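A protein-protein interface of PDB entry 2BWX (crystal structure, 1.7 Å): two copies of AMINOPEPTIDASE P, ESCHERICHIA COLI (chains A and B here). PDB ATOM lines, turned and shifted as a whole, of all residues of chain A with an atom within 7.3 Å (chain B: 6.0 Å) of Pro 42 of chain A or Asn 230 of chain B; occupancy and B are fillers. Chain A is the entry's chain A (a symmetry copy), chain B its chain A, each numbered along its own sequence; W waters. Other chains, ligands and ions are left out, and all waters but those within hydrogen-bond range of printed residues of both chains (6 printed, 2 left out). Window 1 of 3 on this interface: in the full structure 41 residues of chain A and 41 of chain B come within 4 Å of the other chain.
O of Pro 42 of chain A is in hydrogen-bond range of OH of Tyr 41 of chain B (2.6 Å). The side-chain amide nitrogen (ND2) of Asn 230 of chain B lies within hydrogen-bond range of the backbone carbonyl oxygen (O) of Glu 40 of chain A (2.9 Å). O of Thr 245 of chain B sits at hydrogen-bond distance from NH2 of Arg 225 of chain A, 2.9 Å away.
The backbone carbonyl oxygen (O) of Val 33 of chain A is in hydrogen-bond range of the backbone NH (N) of Tyr 41 of chain A (2.9 Å). NH2 of Arg 225 of chain A lies close to OH of Tyr 226 of chain A (3.4 Å).
Arg 35 of chain A touches Pro 227 of chain B (NH1 to O, 3.7 Å). CD1 of Tyr 41 of chain A touches CD1 of Tyr 41 of chain B, 3.3 Å away. C of Tyr 41 of chain A touches ND2 of Asn 230 of chain B, 3.7 Å away. Pro 42 of chain A touches Asn 230 of chain B (CD to OD1, 3.3 Å). Arg 44 of chain A touches Arg 35 of chain B (CG to O, 3.5 Å). Arg 44 of chain A touches Tyr 41 of chain B (N to OH, 3.6 Å). Tyr 226 of chain A touches Arg 35 of chain B.
Ser 39 of chain A touches none of the printed residues of chain B. Printed residues of chain B within 4 Å of Glu 40 of chain A: Asn 230. Of chain B, only Tyr 41 and Asn 230 come within 4 Å of Pro 42 of chain A. Of the printed residues of chain B, Arg 225 of chain A touches Thr 245 (2.9 Å). Printed residues of chain B within 4 Å of Tyr 226 of chain A: Arg 35 (3.9 Å). Printed residues of chain A within 4 Å of Arg 35 of chain B: Arg 44 (3.5 Å) and Tyr 226 (3.9 Å). Of the printed residues of chain A, Asn 230 of chain B touches Glu 40, Tyr 41 and Pro 42. Printed residues of chain A within 4 Å of Thr 245 of chain B: Arg 225 (2.9 Å). The nearest residue of chain B that does not touch Pro 42 of chain A is Arg 35 of chain B (5.3 Å). The nearest printed residue of chain B that does not touch Arg 35 of chain A is Ser 228 of chain B (4.1 Å).
Of the 12 printed residues of chain B, 5 touch a printed residue of chain A. Along chain B the printed residues that touch a printed residue of chain A span positions 35 to 245. Hydrophobic or aromatic side chains of chain A that line the printed part of chain B: Tyr 41, Pro 42 and Tyr 226. Among the printed residues, no Asp or Glu carboxylate lies within 4 Å of a Lys or Arg side-chain nitrogen of the other chain.
Tyr 41 of chain A touches its own counterpart, Tyr 41 of chain B. Of the 10 pairs that touch across the chains among the printed residues, 1 has its exchanged pair printed and touching as well.
Water W6 lies within hydrogen-bond range of the side-chain hydroxyl (OG) of Ser 39 of chain A (2.6 Å), the backbone carbonyl oxygen (O) of Ser 228 of chain B (2.7 Å) and the guanidinium group (NH1) of Arg 35 of chain A (3.0 Å). Water W5 lies within hydrogen-bond range of the backbone carbonyl oxygen of Thr 231 of chain B (2.7 Å), the guanidinium group of Arg 225 of chain A (3.2 Å) and the backbone carbonyl oxygen of Thr 245 of chain B (3.4 Å). Water W3 lies within hydrogen-bond range of OH of Tyr 41 of chain B (2.7 Å) and N of Arg 44 of chain A (3.1 Å). Water W4 bridges O of Tyr 43 of chain A (2.8 Å) and NH2 of Arg 35 of chain B (3.0 Å). Water W2 bridges N of Asn 230 of chain B and O of Glu 40 of chain A. Water W1 lies within hydrogen-bond range of the backbone carbonyl oxygen (O) of Glu 40 of chain A and the side-chain amide oxygen (OD1) of Asn 230 of chain B.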
ATOM      1  N   VAL A  33      36.016  19.322 -13.018  1.00  0.00           N
ATOM      2  CA  VAL A  33      36.804  18.272 -12.371  1.00  0.00           C
ATOM      3  C   VAL A  33      36.350  16.895 -12.905  1.00  0.00           C
ATOM      4  O   VAL A  33      35.185  16.556 -12.821  1.00  0.00           O
ATOM      5  CB  VAL A  33      36.551  18.322 -10.849  1.00  0.00           C
ATOM      6  CG1 VAL A  33      37.269  17.266 -10.177  1.00  0.00           C
ATOM      7  CG2 VAL A  33      36.986  19.642 -10.269  1.00  0.00           C
ATOM      8  N   ARG A  35      35.645  13.014 -12.925  1.00  0.00           N
ATOM      9  CA  ARG A  35      35.368  11.894 -12.053  1.00  0.00           C
ATOM     10  C   ARG A  35      36.031  10.626 -12.603  1.00  0.00           C
ATOM     11  O   ARG A  35      36.764   9.935 -11.890  1.00  0.00           O
ATOM     12  CB  ARG A  35      33.857  11.677 -11.873  1.00  0.00           C
ATOM     13  CG  ARG A  35      33.560  10.518 -10.961  1.00  0.00           C
ATOM     14  CD  ARG A  35      32.128  10.483 -10.475  1.00  0.00           C
ATOM     15  NE  ARG A  35      31.941   9.375  -9.536  1.00  0.00           N
ATOM     16  CZ  ARG A  35      31.686   8.115  -9.860  1.00  0.00           C
ATOM     17  NH1 ARG A  35      31.522   7.740 -11.124  1.00  0.00           N
ATOM     18  NH2 ARG A  35      31.572   7.209  -8.902  1.00  0.00           N
ATOM     19  N   SER A  39      33.648  11.686 -17.890  1.00  0.00           N
ATOM     20  CA  SER A  39      32.594  12.150 -17.000  1.00  0.00           C
ATOM     21  C   SER A  39      33.169  13.052 -15.911  1.00  0.00           C
ATOM     22  O   SER A  39      34.195  12.727 -15.294  1.00  0.00           O
ATOM     23  CB  SER A  39      31.853  10.976 -16.376  1.00  0.00           C
ATOM     24  OG  SER A  39      32.700  10.268 -15.493  1.00  0.00           O
ATOM     25  N   GLU A  40      32.513  14.187 -15.698  1.00  0.00           N
ATOM     26  CA  GLU A  40      32.915  15.140 -14.666  1.00  0.00           C
ATOM     27  C   GLU A  40      32.027  15.014 -13.437  1.00  0.00           C
ATOM     28  O   GLU A  40      30.874  14.551 -13.523  1.00  0.00           O
ATOM     29  CB  GLU A  40      32.874  16.563 -15.214  1.00  0.00           C
ATOM     30  CG  GLU A  40      33.853  16.771 -16.378  1.00  0.00           C
ATOM     31  CD  GLU A  40      33.484  17.929 -17.294  1.00  0.00           C
ATOM     32  OE1 GLU A  40      32.463  18.615 -17.044  1.00  0.00           O
ATOM     33  OE2 GLU A  40      34.228  18.153 -18.269  1.00  0.00           O
ATOM     34  N   TYR A  41      32.573  15.403 -12.297  1.00  0.00           N
ATOM     35  CA  TYR A  41      31.811  15.540 -11.074  1.00  0.00           C
ATOM     36  C   TYR A  41      30.803  16.681 -11.280  1.00  0.00           C
ATOM     37  O   TYR A  41      31.052  17.575 -12.089  1.00  0.00           O
ATOM     38  CB  TYR A  41      32.729  15.893  -9.902  1.00  0.00           C
ATOM     39  CG  TYR A  41      33.444  14.717  -9.288  1.00  0.00           C
ATOM     40  CD1 TYR A  41      32.772  13.821  -8.461  1.00  0.00           C
ATOM     41  CD2 TYR A  41      34.804  14.515  -9.509  1.00  0.00           C
ATOM     42  CE1 TYR A  41      33.429  12.723  -7.893  1.00  0.00           C
ATOM     43  CE2 TYR A  41      35.470  13.437  -8.945  1.00  0.00           C
ATOM     44  CZ  TYR A  41      34.788  12.548  -8.127  1.00  0.00           C
ATOM     45  OH  TYR A  41      35.451  11.470  -7.556  1.00  0.00           O
ATOM     46  N   PRO A  42      29.696  16.667 -10.529  1.00  0.00           N
ATOM     47  CA  PRO A  42      28.787  17.825 -10.542  1.00  0.00           C
ATOM     48  C   PRO A  42      29.567  19.087 -10.141  1.00  0.00           C
ATOM     49  O   PRO A  42      30.369  19.063  -9.186  1.00  0.00           O
ATOM     50  CB  PRO A  42      27.737  17.488  -9.471  1.00  0.00           C
ATOM     51  CG  PRO A  42      27.855  16.029  -9.241  1.00  0.00           C
ATOM     52  CD  PRO A  42      29.267  15.638  -9.570  1.00  0.00           C
ATOM     53  N   TYR A  43      29.358  20.158 -10.894  1.00  0.00           N
ATOM     54  CA  TYR A  43      30.176  21.366 -10.772  1.00  0.00           C
ATOM     55  C   TYR A  43      29.950  22.041  -9.423  1.00  0.00           C
ATOM     56  O   TYR A  43      28.816  22.154  -8.951  1.00  0.00           O
ATOM     57  CB  TYR A  43      29.875  22.362 -11.887  1.00  0.00           C
ATOM     58  CG  TYR A  43      30.798  23.551 -11.885  1.00  0.00           C
ATOM     59  CD1 TYR A  43      32.153  23.398 -12.142  1.00  0.00           C
ATOM     60  CD2 TYR A  43      30.324  24.850 -11.597  1.00  0.00           C
ATOM     61  CE1 TYR A  43      33.027  24.494 -12.134  1.00  0.00           C
ATOM     62  CE2 TYR A  43      31.172  25.944 -11.608  1.00  0.00           C
ATOM     63  CZ  TYR A  43      32.527  25.775 -11.870  1.00  0.00           C
ATOM     64  OH  TYR A  43      33.377  26.861 -11.882  1.00  0.00           O
ATOM     65  N   ARG A  44      31.046  22.397  -8.773  1.00  0.00           N
ATOM     66  CA  ARG A  44      31.002  23.224  -7.570  1.00  0.00           C
ATOM     67  C   ARG A  44      31.831  24.483  -7.795  1.00  0.00           C
ATOM     68  O   ARG A  44      33.067  24.422  -8.008  1.00  0.00           O
ATOM     69  CB  ARG A  44      31.510  22.431  -6.355  1.00  0.00           C
ATOM     70  CG  ARG A  44      31.705  23.281  -5.098  1.00  0.00           C
ATOM     71  CD  ARG A  44      30.442  24.067  -4.677  1.00  0.00           C
ATOM     72  NE  ARG A  44      30.414  24.202  -3.215  1.00  0.00           N
ATOM     73  CZ  ARG A  44      31.199  25.025  -2.513  1.00  0.00           C
ATOM     74  NH1 ARG A  44      32.054  25.831  -3.120  1.00  0.00           N
ATOM     75  NH2 ARG A  44      31.142  25.037  -1.178  1.00  0.00           N
ATOM     76  N   GLN A  45      31.151  25.621  -7.785  1.00  0.00           N
ATOM     77  CA  GLN A  45      31.817  26.897  -8.003  1.00  0.00           C
ATOM     78  C   GLN A  45      32.761  27.175  -6.826  1.00  0.00           C
ATOM     79  O   GLN A  45      32.489  26.767  -5.682  1.00  0.00           O
ATOM     80  CB  GLN A  45      30.779  28.030  -8.142  1.00  0.00           C
ATOM     81  CG  GLN A  45      31.362  29.388  -8.521  1.00  0.00           C
ATOM     82  CD  GLN A  45      32.248  29.320  -9.751  1.00  0.00           C
ATOM     83  OE1 GLN A  45      33.465  29.101  -9.650  1.00  0.00           O
ATOM     84  NE2 GLN A  45      31.645  29.533 -10.912  1.00  0.00           N
ATOM     85  N   ARG A 225      20.361  20.081  -3.428  1.00  0.00           N
ATOM     86  CA  ARG A 225      20.686  18.894  -4.237  1.00  0.00           C
ATOM     87  C   ARG A 225      21.900  18.150  -3.726  1.00  0.00           C
ATOM     88  O   ARG A 225      21.941  16.929  -3.775  1.00  0.00           O
ATOM     89  CB  ARG A 225      20.938  19.248  -5.707  1.00  0.00           C
ATOM     90  CG  ARG A 225      19.700  19.596  -6.492  1.00  0.00           C
ATOM     91  CD  ARG A 225      20.106  20.136  -7.854  1.00  0.00           C
ATOM     92  NE  ARG A 225      20.434  19.080  -8.800  1.00  0.00           N
ATOM     93  CZ  ARG A 225      21.119  19.256  -9.928  1.00  0.00           C
ATOM     94  NH1 ARG A 225      21.627  20.444 -10.245  1.00  0.00           N
ATOM     95  NH2 ARG A 225      21.310  18.236 -10.747  1.00  0.00           N
ATOM     96  N   TYR A 226      22.899  18.893  -3.265  1.00  0.00           N
ATOM     97  CA  TYR A 226      24.190  18.322  -2.889  1.00  0.00           C
ATOM     98  C   TYR A 226      24.504  18.504  -1.419  1.00  0.00           C
ATOM     99  O   TYR A 226      24.248  19.576  -0.848  1.00  0.00           O
ATOM    100  CB  TYR A 226      25.324  18.948  -3.699  1.00  0.00           C
ATOM    101  CG  TYR A 226      25.090  18.865  -5.196  1.00  0.00           C
ATOM    102  CD1 TYR A 226      25.047  17.636  -5.840  1.00  0.00           C
ATOM    103  CD2 TYR A 226      24.861  20.004  -5.945  1.00  0.00           C
ATOM    104  CE1 TYR A 226      24.805  17.546  -7.212  1.00  0.00           C
ATOM    105  CE2 TYR A 226      24.612  19.924  -7.325  1.00  0.00           C
ATOM    106  CZ  TYR A 226      24.598  18.688  -7.940  1.00  0.00           C
ATOM    107  OH  TYR A 226      24.343  18.595  -9.295  1.00  0.00           O
ATOM    108  N   ARG B  35      36.615  19.245  -3.928  1.00  0.00           N
ATOM    109  CA  ARG B  35      35.336  19.831  -4.263  1.00  0.00           C
ATOM    110  C   ARG B  35      35.349  21.330  -3.945  1.00  0.00           C
ATOM    111  O   ARG B  35      35.018  22.160  -4.799  1.00  0.00           O
ATOM    112  CB  ARG B  35      34.183  19.133  -3.522  1.00  0.00           C
ATOM    113  CG  ARG B  35      32.848  19.732  -3.870  1.00  0.00           C
ATOM    114  CD  ARG B  35      31.674  18.871  -3.455  1.00  0.00           C
ATOM    115  NE  ARG B  35      30.419  19.485  -3.896  1.00  0.00           N
ATOM    116  CZ  ARG B  35      29.743  20.425  -3.250  1.00  0.00           C
ATOM    117  NH1 ARG B  35      30.141  20.881  -2.066  1.00  0.00           N
ATOM    118  NH2 ARG B  35      28.636  20.912  -3.786  1.00  0.00           N
ATOM    119  N   TYR B  41      35.697  15.486  -3.178  1.00  0.00           N
ATOM    120  CA  TYR B  41      34.620  14.717  -3.764  1.00  0.00           C
ATOM    121  C   TYR B  41      34.746  13.273  -3.254  1.00  0.00           C
ATOM    122  O   TYR B  41      35.848  12.843  -2.912  1.00  0.00           O
ATOM    123  CB  TYR B  41      34.727  14.716  -5.291  1.00  0.00           C
ATOM    124  CG  TYR B  41      34.172  15.947  -5.960  1.00  0.00           C
ATOM    125  CD1 TYR B  41      32.798  16.141  -6.080  1.00  0.00           C
ATOM    126  CD2 TYR B  41      35.021  16.908  -6.503  1.00  0.00           C
ATOM    127  CE1 TYR B  41      32.276  17.286  -6.695  1.00  0.00           C
ATOM    128  CE2 TYR B  41      34.519  18.042  -7.123  1.00  0.00           C
ATOM    129  CZ  TYR B  41      33.148  18.226  -7.231  1.00  0.00           C
ATOM    130  OH  TYR B  41      32.639  19.357  -7.856  1.00  0.00           O
ATOM    131  N   HIS B 216      18.342   8.578  -7.241  1.00  0.00           N
ATOM    132  CA  HIS B 216      19.536   8.369  -6.426  1.00  0.00           C
ATOM    133  C   HIS B 216      19.226   7.565  -5.160  1.00  0.00           C
ATOM    134  O   HIS B 216      20.061   6.752  -4.722  1.00  0.00           O
ATOM    135  CB  HIS B 216      20.186   9.697  -6.077  1.00  0.00           C
ATOM    136  CG  HIS B 216      20.759  10.409  -7.264  1.00  0.00           C
ATOM    137  ND1 HIS B 216      21.233  11.699  -7.187  1.00  0.00           N
ATOM    138  CD2 HIS B 216      20.927  10.018  -8.547  1.00  0.00           C
ATOM    139  CE1 HIS B 216      21.689  12.065  -8.375  1.00  0.00           C
ATOM    140  NE2 HIS B 216      21.528  11.062  -9.213  1.00  0.00           N
ATOM    141  N   PRO B 227      25.858   7.471  -8.691  1.00  0.00           N
ATOM    142  CA  PRO B 227      25.547   7.373 -10.119  1.00  0.00           C
ATOM    143  C   PRO B 227      26.822   7.220 -10.956  1.00  0.00           C
ATOM    144  O   PRO B 227      27.892   7.669 -10.548  1.00  0.00           O
ATOM    145  CB  PRO B 227      24.910   8.718 -10.443  1.00  0.00           C
ATOM    146  CG  PRO B 227      24.615   9.357  -9.151  1.00  0.00           C
ATOM    147  CD  PRO B 227      25.569   8.822  -8.171  1.00  0.00           C
ATOM    148  N   SER B 228      26.694   6.599 -12.118  1.00  0.00           N
ATOM    149  CA  SER B 228      27.821   6.457 -13.036  1.00  0.00           C
ATOM    150  C   SER B 228      28.118   7.725 -13.848  1.00  0.00           C
ATOM    151  O   SER B 228      29.169   7.823 -14.471  1.00  0.00           O
ATOM    152  CB  SER B 228      27.573   5.275 -13.988  1.00  0.00           C
ATOM    153  OG  SER B 228      26.293   5.352 -14.607  1.00  0.00           O
ATOM    154  N   TYR B 229      27.189   8.676 -13.833  1.00  0.00           N
ATOM    155  CA  TYR B 229      27.352   9.970 -14.494  1.00  0.00           C
ATOM    156  C   TYR B 229      26.279  10.893 -13.938  1.00  0.00           C
ATOM    157  O   TYR B 229      25.351  10.426 -13.285  1.00  0.00           O
ATOM    158  CB  TYR B 229      27.205   9.858 -16.015  1.00  0.00           C
ATOM    159  CG  TYR B 229      25.940   9.167 -16.450  1.00  0.00           C
ATOM    160  CD1 TYR B 229      25.892   7.783 -16.582  1.00  0.00           C
ATOM    161  CD2 TYR B 229      24.763   9.895 -16.712  1.00  0.00           C
ATOM    162  CE1 TYR B 229      24.729   7.137 -16.958  1.00  0.00           C
ATOM    163  CE2 TYR B 229      23.587   9.252 -17.112  1.00  0.00           C
ATOM    164  CZ  TYR B 229      23.573   7.868 -17.240  1.00  0.00           C
ATOM    165  OH  TYR B 229      22.438   7.196 -17.619  1.00  0.00           O
ATOM    166  N   ASN B 230      26.408  12.184 -14.195  1.00  0.00           N
ATOM    167  CA  ASN B 230      25.457  13.144 -13.631  1.00  0.00           C
ATOM    168  C   ASN B 230      24.075  12.984 -14.261  1.00  0.00           C
ATOM    169  O   ASN B 230      23.915  13.048 -15.480  1.00  0.00           O
ATOM    170  CB  ASN B 230      25.971  14.577 -13.793  1.00  0.00           C
ATOM    171  CG  ASN B 230      27.298  14.795 -13.089  1.00  0.00           C
ATOM    172  OD1 ASN B 230      27.555  14.206 -12.036  1.00  0.00           O
ATOM    173  ND2 ASN B 230      28.136  15.637 -13.659  1.00  0.00           N
ATOM    174  N   THR B 231      23.093  12.706 -13.408  1.00  0.00           N
ATOM    175  CA  THR B 231      21.717  12.480 -13.836  1.00  0.00           C
ATOM    176  C   THR B 231      21.143  13.666 -14.613  1.00  0.00           C
ATOM    177  O   THR B 231      21.279  14.830 -14.203  1.00  0.00           O
ATOM    178  CB  THR B 231      20.847  12.176 -12.596  1.00  0.00           C
ATOM    179  OG1 THR B 231      21.333  10.975 -11.993  1.00  0.00           O
ATOM    180  CG2 THR B 231      19.382  12.056 -12.945  1.00  0.00           C
ATOM    181  N   ILE B 232      20.474  13.337 -15.715  1.00  0.00           N
ATOM    182  CA  ILE B 232      19.821  14.291 -16.614  1.00  0.00           C
ATOM    183  C   ILE B 232      18.304  14.135 -16.439  1.00  0.00           C
ATOM    184  O   ILE B 232      17.763  13.040 -16.603  1.00  0.00           O
ATOM    185  CB  ILE B 232      20.202  13.961 -18.082  1.00  0.00           C
ATOM    186  CG1 ILE B 232      21.697  14.208 -18.307  1.00  0.00           C
ATOM    187  CG2 ILE B 232      19.333  14.718 -19.100  1.00  0.00           C
ATOM    188  CD1 ILE B 232      22.300  13.411 -19.472  1.00  0.00           C
ATOM    189  N   TYR B 244      21.710  17.946 -20.319  1.00  0.00           N
ATOM    190  CA  TYR B 244      21.070  18.869 -19.393  1.00  0.00           C
ATOM    191  C   TYR B 244      21.130  18.289 -17.975  1.00  0.00           C
ATOM    192  O   TYR B 244      20.482  17.288 -17.702  1.00  0.00           O
ATOM    193  CB  TYR B 244      19.604  19.069 -19.804  1.00  0.00           C
ATOM    194  CG  TYR B 244      18.829  19.935 -18.845  1.00  0.00           C
ATOM    195  CD1 TYR B 244      18.963  21.325 -18.863  1.00  0.00           C
ATOM    196  CD2 TYR B 244      17.969  19.358 -17.901  1.00  0.00           C
ATOM    197  CE1 TYR B 244      18.249  22.126 -17.982  1.00  0.00           C
ATOM    198  CE2 TYR B 244      17.258  20.147 -17.018  1.00  0.00           C
ATOM    199  CZ  TYR B 244      17.390  21.530 -17.061  1.00  0.00           C
ATOM    200  OH  TYR B 244      16.682  22.305 -16.173  1.00  0.00           O
ATOM    201  N   THR B 245      21.905  18.909 -17.084  1.00  0.00           N
ATOM    202  CA  THR B 245      22.021  18.400 -15.712  1.00  0.00           C
ATOM    203  C   THR B 245      21.656  19.437 -14.646  1.00  0.00           C
ATOM    204  O   THR B 245      21.713  19.125 -13.452  1.00  0.00           O
ATOM    205  CB  THR B 245      23.440  17.874 -15.432  1.00  0.00           C
ATOM    206  OG1 THR B 245      24.384  18.944 -15.620  1.00  0.00           O
ATOM    207  CG2 THR B 245      23.770  16.675 -16.344  1.00  0.00           C
ATOM    208  N   ASP B 260      17.863  10.598 -18.194  1.00  0.00           N
ATOM    209  CA  ASP B 260      19.040   9.808 -18.527  1.00  0.00           C
ATOM    210  C   ASP B 260      19.820   9.647 -17.218  1.00  0.00           C
ATOM    211  O   ASP B 260      20.304  10.627 -16.631  1.00  0.00           O
ATOM    212  CB  ASP B 260      19.863  10.500 -19.604  1.00  0.00           C
ATOM    213  CG  ASP B 260      20.927   9.584 -20.229  1.00  0.00           C
ATOM    214  OD1 ASP B 260      21.323   8.555 -19.625  1.00  0.00           O
ATOM    215  OD2 ASP B 260      21.369   9.912 -21.358  1.00  0.00           O
HETATM  216  O   HOH W   1      29.743  11.857 -12.280  1.00  0.00           O
HETATM  217  O   HOH W   2      29.023  12.967 -15.305  1.00  0.00           O
HETATM  218  O   HOH W   3      33.553  20.949  -9.861  1.00  0.00           O
HETATM  219  O   HOH W   4      27.890  20.736  -6.712  1.00  0.00           O
HETATM  220  O   HOH W   5      22.882  16.095 -12.482  1.00  0.00           O
HETATM  221  O   HOH W   6      31.164   9.484 -13.579  1.00  0.00           O
